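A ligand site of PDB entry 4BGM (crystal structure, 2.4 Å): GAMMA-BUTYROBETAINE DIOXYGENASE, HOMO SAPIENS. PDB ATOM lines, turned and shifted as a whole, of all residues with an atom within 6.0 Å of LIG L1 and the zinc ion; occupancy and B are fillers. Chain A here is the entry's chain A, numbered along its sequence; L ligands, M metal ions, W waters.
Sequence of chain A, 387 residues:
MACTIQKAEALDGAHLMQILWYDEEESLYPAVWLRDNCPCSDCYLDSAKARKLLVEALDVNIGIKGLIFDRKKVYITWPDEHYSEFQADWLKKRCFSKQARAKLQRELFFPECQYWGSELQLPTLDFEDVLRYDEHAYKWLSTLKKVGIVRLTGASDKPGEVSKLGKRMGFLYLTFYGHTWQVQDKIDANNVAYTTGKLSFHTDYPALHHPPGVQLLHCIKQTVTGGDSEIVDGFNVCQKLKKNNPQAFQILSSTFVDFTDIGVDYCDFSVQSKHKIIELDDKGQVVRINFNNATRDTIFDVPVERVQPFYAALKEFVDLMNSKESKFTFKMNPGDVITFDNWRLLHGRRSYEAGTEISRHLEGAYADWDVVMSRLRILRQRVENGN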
ATOM      1  N   TRP A 181       3.150 -16.278   6.728  1.00  0.00           N
ATOM      2  CA  TRP A 181       2.973 -17.609   6.205  1.00  0.00           C
ATOM      3  C   TRP A 181       1.693 -17.670   5.414  1.00  0.00           C
ATOM      4  O   TRP A 181       0.785 -16.866   5.637  1.00  0.00           O
ATOM      5  CB  TRP A 181       2.949 -18.671   7.311  1.00  0.00           C
ATOM      6  CG  TRP A 181       2.526 -18.188   8.629  1.00  0.00           C
ATOM      7  CD1 TRP A 181       3.329 -17.729   9.620  1.00  0.00           C
ATOM      8  CD2 TRP A 181       1.183 -18.126   9.132  1.00  0.00           C
ATOM      9  NE1 TRP A 181       2.574 -17.374  10.711  1.00  0.00           N
ATOM     10  CE2 TRP A 181       1.249 -17.606  10.435  1.00  0.00           C
ATOM     11  CE3 TRP A 181      -0.078 -18.459   8.610  1.00  0.00           C
ATOM     12  CZ2 TRP A 181       0.125 -17.428  11.215  1.00  0.00           C
ATOM     13  CZ3 TRP A 181      -1.194 -18.270   9.387  1.00  0.00           C
ATOM     14  CH2 TRP A 181      -1.081 -17.771  10.673  1.00  0.00           C
ATOM     15  N   VAL A 183      -1.601 -19.657   4.135  1.00  0.00           N
ATOM     16  CA  VAL A 183      -2.561 -20.727   4.454  1.00  0.00           C
ATOM     17  C   VAL A 183      -3.325 -21.076   3.189  1.00  0.00           C
ATOM     18  O   VAL A 183      -4.195 -20.337   2.747  1.00  0.00           O
ATOM     19  CB  VAL A 183      -3.552 -20.325   5.557  1.00  0.00           C
ATOM     20  CG1 VAL A 183      -4.527 -21.454   5.884  1.00  0.00           C
ATOM     21  CG2 VAL A 183      -2.783 -19.929   6.798  1.00  0.00           C
ATOM     22  N   ASN A 191       1.663 -29.359   7.652  1.00  0.00           N
ATOM     23  CA  ASN A 191       0.751 -28.883   8.694  1.00  0.00           C
ATOM     24  C   ASN A 191      -0.706 -28.983   8.240  1.00  0.00           C
ATOM     25  O   ASN A 191      -1.012 -28.644   7.108  1.00  0.00           O
ATOM     26  CB  ASN A 191       1.115 -27.437   9.052  1.00  0.00           C
ATOM     27  CG  ASN A 191       0.512 -26.968  10.382  1.00  0.00           C
ATOM     28  OD1 ASN A 191      -0.673 -26.722  10.467  1.00  0.00           O
ATOM     29  ND2 ASN A 191       1.341 -26.812  11.389  1.00  0.00           N
ATOM     30  N   ALA A 193      -3.195 -27.228   8.702  1.00  0.00           N
ATOM     31  CA  ALA A 193      -3.718 -25.942   8.232  1.00  0.00           C
ATOM     32  C   ALA A 193      -3.555 -25.784   6.720  1.00  0.00           C
ATOM     33  O   ALA A 193      -4.341 -25.102   6.065  1.00  0.00           O
ATOM     34  CB  ALA A 193      -3.032 -24.819   8.965  1.00  0.00           C
ATOM     35  N   TYR A 194      -2.516 -26.421   6.176  1.00  0.00           N
ATOM     36  CA  TYR A 194      -2.199 -26.372   4.770  1.00  0.00           C
ATOM     37  C   TYR A 194      -2.846 -27.551   3.936  1.00  0.00           C
ATOM     38  O   TYR A 194      -2.197 -28.193   3.100  1.00  0.00           O
ATOM     39  CB  TYR A 194      -0.668 -26.346   4.612  1.00  0.00           C
ATOM     40  CG  TYR A 194       0.057 -25.211   5.377  1.00  0.00           C
ATOM     41  CD1 TYR A 194      -0.593 -23.983   5.709  1.00  0.00           C
ATOM     42  CD2 TYR A 194       1.416 -25.335   5.715  1.00  0.00           C
ATOM     43  CE1 TYR A 194       0.084 -22.964   6.375  1.00  0.00           C
ATOM     44  CE2 TYR A 194       2.087 -24.305   6.363  1.00  0.00           C
ATOM     45  CZ  TYR A 194       1.423 -23.132   6.680  1.00  0.00           C
ATOM     46  OH  TYR A 194       2.109 -22.143   7.314  1.00  0.00           O
ATOM     47  N   LEU A 199     -10.681 -27.569  10.391  1.00  0.00           N
ATOM     48  CA  LEU A 199      -9.924 -27.368  11.600  1.00  0.00           C
ATOM     49  C   LEU A 199     -10.953 -27.085  12.675  1.00  0.00           C
ATOM     50  O   LEU A 199     -11.713 -26.141  12.549  1.00  0.00           O
ATOM     51  CB  LEU A 199      -8.977 -26.177  11.452  1.00  0.00           C
ATOM     52  CG  LEU A 199      -8.015 -26.289  10.288  1.00  0.00           C
ATOM     53  CD1 LEU A 199      -7.297 -24.975  10.102  1.00  0.00           C
ATOM     54  CD2 LEU A 199      -7.002 -27.408  10.517  1.00  0.00           C
ATOM     55  N   HIS A 202      -9.059 -24.524  17.991  1.00  0.00           N
ATOM     56  CA  HIS A 202      -7.714 -24.649  18.517  1.00  0.00           C
ATOM     57  C   HIS A 202      -7.140 -23.269  18.796  1.00  0.00           C
ATOM     58  O   HIS A 202      -7.697 -22.252  18.329  1.00  0.00           O
ATOM     59  CB  HIS A 202      -6.797 -25.375  17.502  1.00  0.00           C
ATOM     60  CG  HIS A 202      -6.632 -24.653  16.194  1.00  0.00           C
ATOM     61  ND1 HIS A 202      -7.625 -24.609  15.251  1.00  0.00           N
ATOM     62  CD2 HIS A 202      -5.598 -23.951  15.682  1.00  0.00           C
ATOM     63  CE1 HIS A 202      -7.212 -23.914  14.202  1.00  0.00           C
ATOM     64  NE2 HIS A 202      -5.986 -23.496  14.446  1.00  0.00           N
ATOM     65  N   THR A 203      -6.038 -23.236  19.525  1.00  0.00           N
ATOM     66  CA  THR A 203      -5.180 -22.070  19.560  1.00  0.00           C
ATOM     67  C   THR A 203      -4.012 -22.444  18.724  1.00  0.00           C
ATOM     68  O   THR A 203      -3.776 -23.609  18.534  1.00  0.00           O
ATOM     69  CB  THR A 203      -4.728 -21.695  20.996  1.00  0.00           C
ATOM     70  OG1 THR A 203      -3.963 -22.746  21.608  1.00  0.00           O
ATOM     71  CG2 THR A 203      -5.934 -21.397  21.851  1.00  0.00           C
ATOM     72  N   ASP A 204      -3.276 -21.460  18.219  1.00  0.00           N
ATOM     73  CA  ASP A 204      -2.112 -21.699  17.364  1.00  0.00           C
ATOM     74  C   ASP A 204      -0.858 -21.791  18.194  1.00  0.00           C
ATOM     75  O   ASP A 204      -0.676 -21.043  19.151  1.00  0.00           O
ATOM     76  CB  ASP A 204      -1.942 -20.579  16.347  1.00  0.00           C
ATOM     77  CG  ASP A 204      -2.597 -20.891  15.002  1.00  0.00           C
ATOM     78  OD1 ASP A 204      -3.629 -21.639  14.954  1.00  0.00           O
ATOM     79  OD2 ASP A 204      -2.082 -20.318  14.010  1.00  0.00           O
ATOM     80  N   GLN A 215      -2.800 -13.067  16.736  1.00  0.00           N
ATOM     81  CA  GLN A 215      -2.741 -13.659  15.412  1.00  0.00           C
ATOM     82  C   GLN A 215      -3.394 -12.732  14.432  1.00  0.00           C
ATOM     83  O   GLN A 215      -4.416 -12.117  14.720  1.00  0.00           O
ATOM     84  CB  GLN A 215      -3.420 -15.042  15.384  1.00  0.00           C
ATOM     85  CG  GLN A 215      -3.361 -15.739  14.021  1.00  0.00           C
ATOM     86  CD  GLN A 215      -3.847 -17.195  14.051  1.00  0.00           C
ATOM     87  OE1 GLN A 215      -4.272 -17.752  13.023  1.00  0.00           O
ATOM     88  NE2 GLN A 215      -3.802 -17.797  15.214  1.00  0.00           N
ATOM     89  N   LEU A 217      -4.739 -12.794  10.390  1.00  0.00           N
ATOM     90  CA  LEU A 217      -5.081 -13.617   9.235  1.00  0.00           C
ATOM     91  C   LEU A 217      -5.765 -12.705   8.235  1.00  0.00           C
ATOM     92  O   LEU A 217      -6.758 -12.035   8.556  1.00  0.00           O
ATOM     93  CB  LEU A 217      -6.066 -14.723   9.601  1.00  0.00           C
ATOM     94  CG  LEU A 217      -5.585 -16.074  10.129  1.00  0.00           C
ATOM     95  CD1 LEU A 217      -6.784 -17.025  10.141  1.00  0.00           C
ATOM     96  CD2 LEU A 217      -4.474 -16.673   9.296  1.00  0.00           C
ATOM     97  N   GLY A 227     -14.976 -23.107   3.858  1.00  0.00           N
ATOM     98  CA  GLY A 227     -13.951 -22.230   4.408  1.00  0.00           C
ATOM     99  C   GLY A 227     -14.421 -21.185   5.396  1.00  0.00           C
ATOM    100  O   GLY A 227     -13.721 -20.202   5.646  1.00  0.00           O
ATOM    101  N   ASP A 228     -15.615 -21.377   5.966  1.00  0.00           N
ATOM    102  CA  ASP A 228     -16.149 -20.427   6.907  1.00  0.00           C
ATOM    103  C   ASP A 228     -15.272 -20.403   8.144  1.00  0.00           C
ATOM    104  O   ASP A 228     -14.718 -21.416   8.512  1.00  0.00           O
ATOM    105  CB  ASP A 228     -17.581 -20.801   7.304  1.00  0.00           C
ATOM    106  CG  ASP A 228     -18.572 -20.629   6.175  1.00  0.00           C
ATOM    107  OD1 ASP A 228     -18.462 -21.378   5.201  1.00  0.00           O
ATOM    108  OD2 ASP A 228     -19.455 -19.760   6.264  1.00  0.00           O
ATOM    109  N   SER A 229     -15.149 -19.246   8.770  1.00  0.00           N
ATOM    110  CA  SER A 229     -14.388 -19.126   9.996  1.00  0.00           C
ATOM    111  C   SER A 229     -15.302 -19.364  11.157  1.00  0.00           C
ATOM    112  O   SER A 229     -16.507 -19.109  11.061  1.00  0.00           O
ATOM    113  CB  SER A 229     -13.743 -17.756  10.109  1.00  0.00           C
ATOM    114  OG  SER A 229     -12.919 -17.511   9.004  1.00  0.00           O
ATOM    115  N   ASN A 292      -4.169 -27.247  20.554  1.00  0.00           N
ATOM    116  CA  ASN A 292      -4.407 -27.581  19.153  1.00  0.00           C
ATOM    117  C   ASN A 292      -4.417 -29.125  19.063  1.00  0.00           C
ATOM    118  O   ASN A 292      -3.465 -29.766  19.441  1.00  0.00           O
ATOM    119  CB  ASN A 292      -3.351 -26.928  18.255  1.00  0.00           C
ATOM    120  CG  ASN A 292      -3.505 -27.302  16.791  1.00  0.00           C
ATOM    121  OD1 ASN A 292      -4.231 -28.237  16.443  1.00  0.00           O
ATOM    122  ND2 ASN A 292      -2.798 -26.594  15.916  1.00  0.00           N
ATOM    123  N   MET A 332     -14.794 -14.973   5.857  1.00  0.00           N
ATOM    124  CA  MET A 332     -13.913 -13.890   5.471  1.00  0.00           C
ATOM    125  C   MET A 332     -14.015 -13.684   3.955  1.00  0.00           C
ATOM    126  O   MET A 332     -14.167 -14.643   3.200  1.00  0.00           O
ATOM    127  CB  MET A 332     -12.471 -14.214   5.854  1.00  0.00           C
ATOM    128  CG  MET A 332     -12.214 -14.379   7.356  1.00  0.00           C
ATOM    129  SD  MET A 332     -10.432 -14.553   7.713  1.00  0.00           S
ATOM    130  CE  MET A 332      -9.949 -12.864   7.361  1.00  0.00           C
ATOM    131  N   ASN A 342      -4.899 -14.874  20.588  1.00  0.00           N
ATOM    132  CA  ASN A 342      -4.624 -16.296  20.437  1.00  0.00           C
ATOM    133  C   ASN A 342      -4.350 -16.996  21.781  1.00  0.00           C
ATOM    134  O   ASN A 342      -4.147 -18.209  21.845  1.00  0.00           O
ATOM    135  CB  ASN A 342      -3.456 -16.469  19.462  1.00  0.00           C
ATOM    136  CG  ASN A 342      -3.134 -17.924  19.178  1.00  0.00           C
ATOM    137  OD1 ASN A 342      -3.869 -18.608  18.482  1.00  0.00           O
ATOM    138  ND2 ASN A 342      -2.011 -18.385  19.692  1.00  0.00           N
ATOM    139  N   HIS A 347     -10.035 -20.817  17.473  1.00  0.00           N
ATOM    140  CA  HIS A 347     -10.560 -20.527  16.179  1.00  0.00           C
ATOM    141  C   HIS A 347     -10.537 -21.744  15.285  1.00  0.00           C
ATOM    142  O   HIS A 347      -9.831 -22.718  15.563  1.00  0.00           O
ATOM    143  CB  HIS A 347      -9.776 -19.404  15.548  1.00  0.00           C
ATOM    144  CG  HIS A 347      -8.343 -19.738  15.321  1.00  0.00           C
ATOM    145  ND1 HIS A 347      -7.404 -19.721  16.323  1.00  0.00           N
ATOM    146  CD2 HIS A 347      -7.693 -20.118  14.193  1.00  0.00           C
ATOM    147  CE1 HIS A 347      -6.234 -20.072  15.833  1.00  0.00           C
ATOM    148  NE2 HIS A 347      -6.379 -20.322  14.545  1.00  0.00           N
ATOM    149  N   GLY A 348     -11.275 -21.669  14.196  1.00  0.00           N
ATOM    150  CA  GLY A 348     -11.496 -22.818  13.393  1.00  0.00           C
ATOM    151  C   GLY A 348     -11.970 -22.493  12.011  1.00  0.00           C
ATOM    152  O   GLY A 348     -12.229 -21.358  11.669  1.00  0.00           O
ATOM    153  N   ARG A 349     -12.077 -23.532  11.205  1.00  0.00           N
ATOM    154  CA  ARG A 349     -12.367 -23.370   9.799  1.00  0.00           C
ATOM    155  C   ARG A 349     -13.104 -24.621   9.290  1.00  0.00           C
ATOM    156  O   ARG A 349     -12.758 -25.762   9.663  1.00  0.00           O
ATOM    157  CB  ARG A 349     -11.064 -23.169   9.030  1.00  0.00           C
ATOM    158  CG  ARG A 349     -11.172 -23.464   7.552  1.00  0.00           C
ATOM    159  CD  ARG A 349      -9.834 -23.623   6.887  1.00  0.00           C
ATOM    160  NE  ARG A 349      -9.266 -24.968   6.861  1.00  0.00           N
ATOM    161  CZ  ARG A 349      -7.970 -25.203   6.652  1.00  0.00           C
ATOM    162  NH1 ARG A 349      -7.117 -24.190   6.510  1.00  0.00           N
ATOM    163  NH2 ARG A 349      -7.497 -26.442   6.611  1.00  0.00           N
ATOM    164  N   ARG A 360      -8.271 -20.933  -2.438  1.00  0.00           N
ATOM    165  CA  ARG A 360      -8.312 -20.311  -1.125  1.00  0.00           C
ATOM    166  C   ARG A 360      -6.906 -20.017  -0.600  1.00  0.00           C
ATOM    167  O   ARG A 360      -6.049 -20.900  -0.575  1.00  0.00           O
ATOM    168  CB  ARG A 360      -9.074 -21.200  -0.141  1.00  0.00           C
ATOM    169  CG  ARG A 360      -9.652 -20.436   1.037  1.00  0.00           C
ATOM    170  CD  ARG A 360      -9.998 -21.398   2.130  1.00  0.00           C
ATOM    171  NE  ARG A 360     -10.586 -20.769   3.309  1.00  0.00           N
ATOM    172  CZ  ARG A 360     -10.018 -20.702   4.517  1.00  0.00           C
ATOM    173  NH1 ARG A 360      -8.800 -21.170   4.740  1.00  0.00           N
ATOM    174  NH2 ARG A 360     -10.671 -20.143   5.528  1.00  0.00           N
ATOM    175  N   LEU A 362      -5.007 -17.506   2.559  1.00  0.00           N
ATOM    176  CA  LEU A 362      -4.875 -16.507   3.602  1.00  0.00           C
ATOM    177  C   LEU A 362      -3.384 -16.240   3.828  1.00  0.00           C
ATOM    178  O   LEU A 362      -2.528 -17.115   3.583  1.00  0.00           O
ATOM    179  CB  LEU A 362      -5.513 -16.968   4.906  1.00  0.00           C
ATOM    180  CG  LEU A 362      -6.910 -17.587   4.973  1.00  0.00           C
ATOM    181  CD1 LEU A 362      -7.257 -17.934   6.398  1.00  0.00           C
ATOM    182  CD2 LEU A 362      -7.998 -16.676   4.415  1.00  0.00           C
ATOM    183  N   TYR A 366       1.993 -13.484  13.407  1.00  0.00           N
ATOM    184  CA  TYR A 366       1.792 -13.419  14.844  1.00  0.00           C
ATOM    185  C   TYR A 366       2.512 -12.207  15.412  1.00  0.00           C
ATOM    186  O   TYR A 366       3.402 -11.643  14.769  1.00  0.00           O
ATOM    187  CB  TYR A 366       2.408 -14.644  15.505  1.00  0.00           C
ATOM    188  CG  TYR A 366       1.831 -15.963  15.101  1.00  0.00           C
ATOM    189  CD1 TYR A 366       0.458 -16.246  15.250  1.00  0.00           C
ATOM    190  CD2 TYR A 366       2.646 -16.962  14.589  1.00  0.00           C
ATOM    191  CE1 TYR A 366      -0.050 -17.483  14.895  1.00  0.00           C
ATOM    192  CE2 TYR A 366       2.153 -18.191  14.244  1.00  0.00           C
ATOM    193  CZ  TYR A 366       0.819 -18.457  14.400  1.00  0.00           C
ATOM    194  OH  TYR A 366       0.367 -19.697  14.019  1.00  0.00           O
HETATM  195  C1  LIG L   1      -4.625 -21.971  10.894  1.00  0.00           C
HETATM  196  C2  LIG L   1      -6.024 -21.580  10.878  1.00  0.00           C
HETATM  197  C3  LIG L   1      -7.958 -20.901   9.669  1.00  0.00           C
HETATM  198  C4  LIG L   1      -8.442 -20.807   8.259  1.00  0.00           C
HETATM  199  O1  LIG L   1      -4.079 -22.204  11.986  1.00  0.00           O
HETATM  200  O2  LIG L   1      -4.002 -22.020   9.793  1.00  0.00           O
HETATM  201  O3  LIG L   1      -6.668 -21.455  11.912  1.00  0.00           O
HETATM  202  O4  LIG L   1      -9.511 -20.211   8.128  1.00  0.00           O
HETATM  203  N1  LIG L   1      -6.568 -21.307   9.711  1.00  0.00           N
HETATM  204  O5  LIG L   1      -7.803 -21.327   7.302  1.00  0.00           O
HETATM  205  C1  LG2 L   2       1.614 -21.877  10.661  1.00  0.00           C
HETATM  206  C2  LG2 L   2       2.036 -20.671  11.485  1.00  0.00           C
HETATM  207  C3  LG2 L   2      -0.791 -21.528  10.793  1.00  0.00           C
HETATM  208  C4  LG2 L   2       0.148 -23.639  10.166  1.00  0.00           C
HETATM  209  C5  LG2 L   2       0.400 -22.907  12.458  1.00  0.00           C
HETATM  210  C6  LG2 L   2      -0.776 -23.803  12.882  1.00  0.00           C
HETATM  211  C7  LG2 L   2      -0.903 -23.906  14.396  1.00  0.00           C
HETATM  212  C8  LG2 L   2      -0.105 -25.023  14.986  1.00  0.00           C
HETATM  213  N1  LG2 L   2       0.319 -22.464  11.050  1.00  0.00           N
HETATM  214  O1  LG2 L   2       0.685 -25.732  14.326  1.00  0.00           O
HETATM  215  F1  LG2 L   2       2.661 -21.081  12.631  1.00  0.00           F
HETATM  216  O2  LG2 L   2      -0.264 -25.180  16.206  1.00  0.00           O
HETATM  217 ZN    ZN M   1      -5.092 -21.658  13.503  1.00  0.00          ZN
HETATM  218  O   HOH W   1     -10.915 -19.175  10.126  1.00  0.00           O
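The side-chain amide nitrogen of Gln 215 lies within hydrogen-bond range of the side-chain carboxylate of Asp 204, at 3.3 Å. The side-chain carboxylate (OD2) of Asp 204 lies within hydrogen-bond range of the side-chain hydroxyl (OH) of Tyr 366, 2.5 Å away. The backbone NH of Asp 204 is in hydrogen-bond range of the side-chain amide oxygen of Asn 342, 2.9 Å away. The backbone carbonyl oxygen of Gly 227 is in hydrogen-bond range of the guanidinium group of Arg 360. The guanidinium group (NH1) of Arg 349 lies within hydrogen-bond range of the backbone carbonyl oxygen (O) of Ala 193, 3.0 Å away. O of Arg 349 sits at hydrogen-bond distance from N of Leu 199, at 2.8 Å. OD1 of Asn 191 lies close to N of Ala 193 (3.1 Å). The backbone carbonyl oxygen (O) of Leu 362 sits at hydrogen-bond distance from the backbone NH (N) of Val 183.
The zinc ion is bound by an oxygen (O1) of LIG L1 (1.9 Å), the side-chain carboxylate of Asp 204 (2.1 Å), a ring nitrogen (NE2) of His 347 (2.1 Å), an oxygen (O3) of LIG L1 (2.2 Å) and a ring nitrogen (NE2) of His 202 (2.3 Å).
Water W1 lies within hydrogen-bond range of an oxygen (O4) of LIG L1 (2.7 Å), the side-chain hydroxyl (OG) of Ser 229 (2.8 Å) and the backbone carbonyl oxygen (O) of Gly 348 (3.0 Å).
NH1 of Arg 360 is in salt-bridge range of O5 of LIG L1, at 2.8 Å. NH1 of Arg 349 lies within salt-bridge range of O5 of LIG L1, 3.0 Å away. O1 of LG2 L2 is in hydrogen-bond range of ND2 of Asn 191 (3.2 Å). ND2 of Asn 292 is in hydrogen-bond range of O2 of LG2 L2 (2.9 Å).
Within 4 Å of the zinc ion: His 202, Asp 204 and His 347. The nearest printed residue that does not touch the zinc ion is Gln 215 (4.02 Å).
Val 183 touches LIG L1. Ala 193 touches LIG L1. CD1 of Leu 199 touches C2 of LIG L1, 3.7 Å away. CD1 of Leu 362 touches O5 of LIG L1, 3.6 Å away. Nine residues have an atom within 4 Å of LIG L1: Val 183, Ala 193, Leu 199, His 202, Asp 204, His 347, Arg 349, Arg 360 and Leu 362. Along chain A the residues within 4 Å of LIG L1 span positions 183 to 362. The nearest printed residue that does not touch LIG L1 is Leu 217 (4.1 Å).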
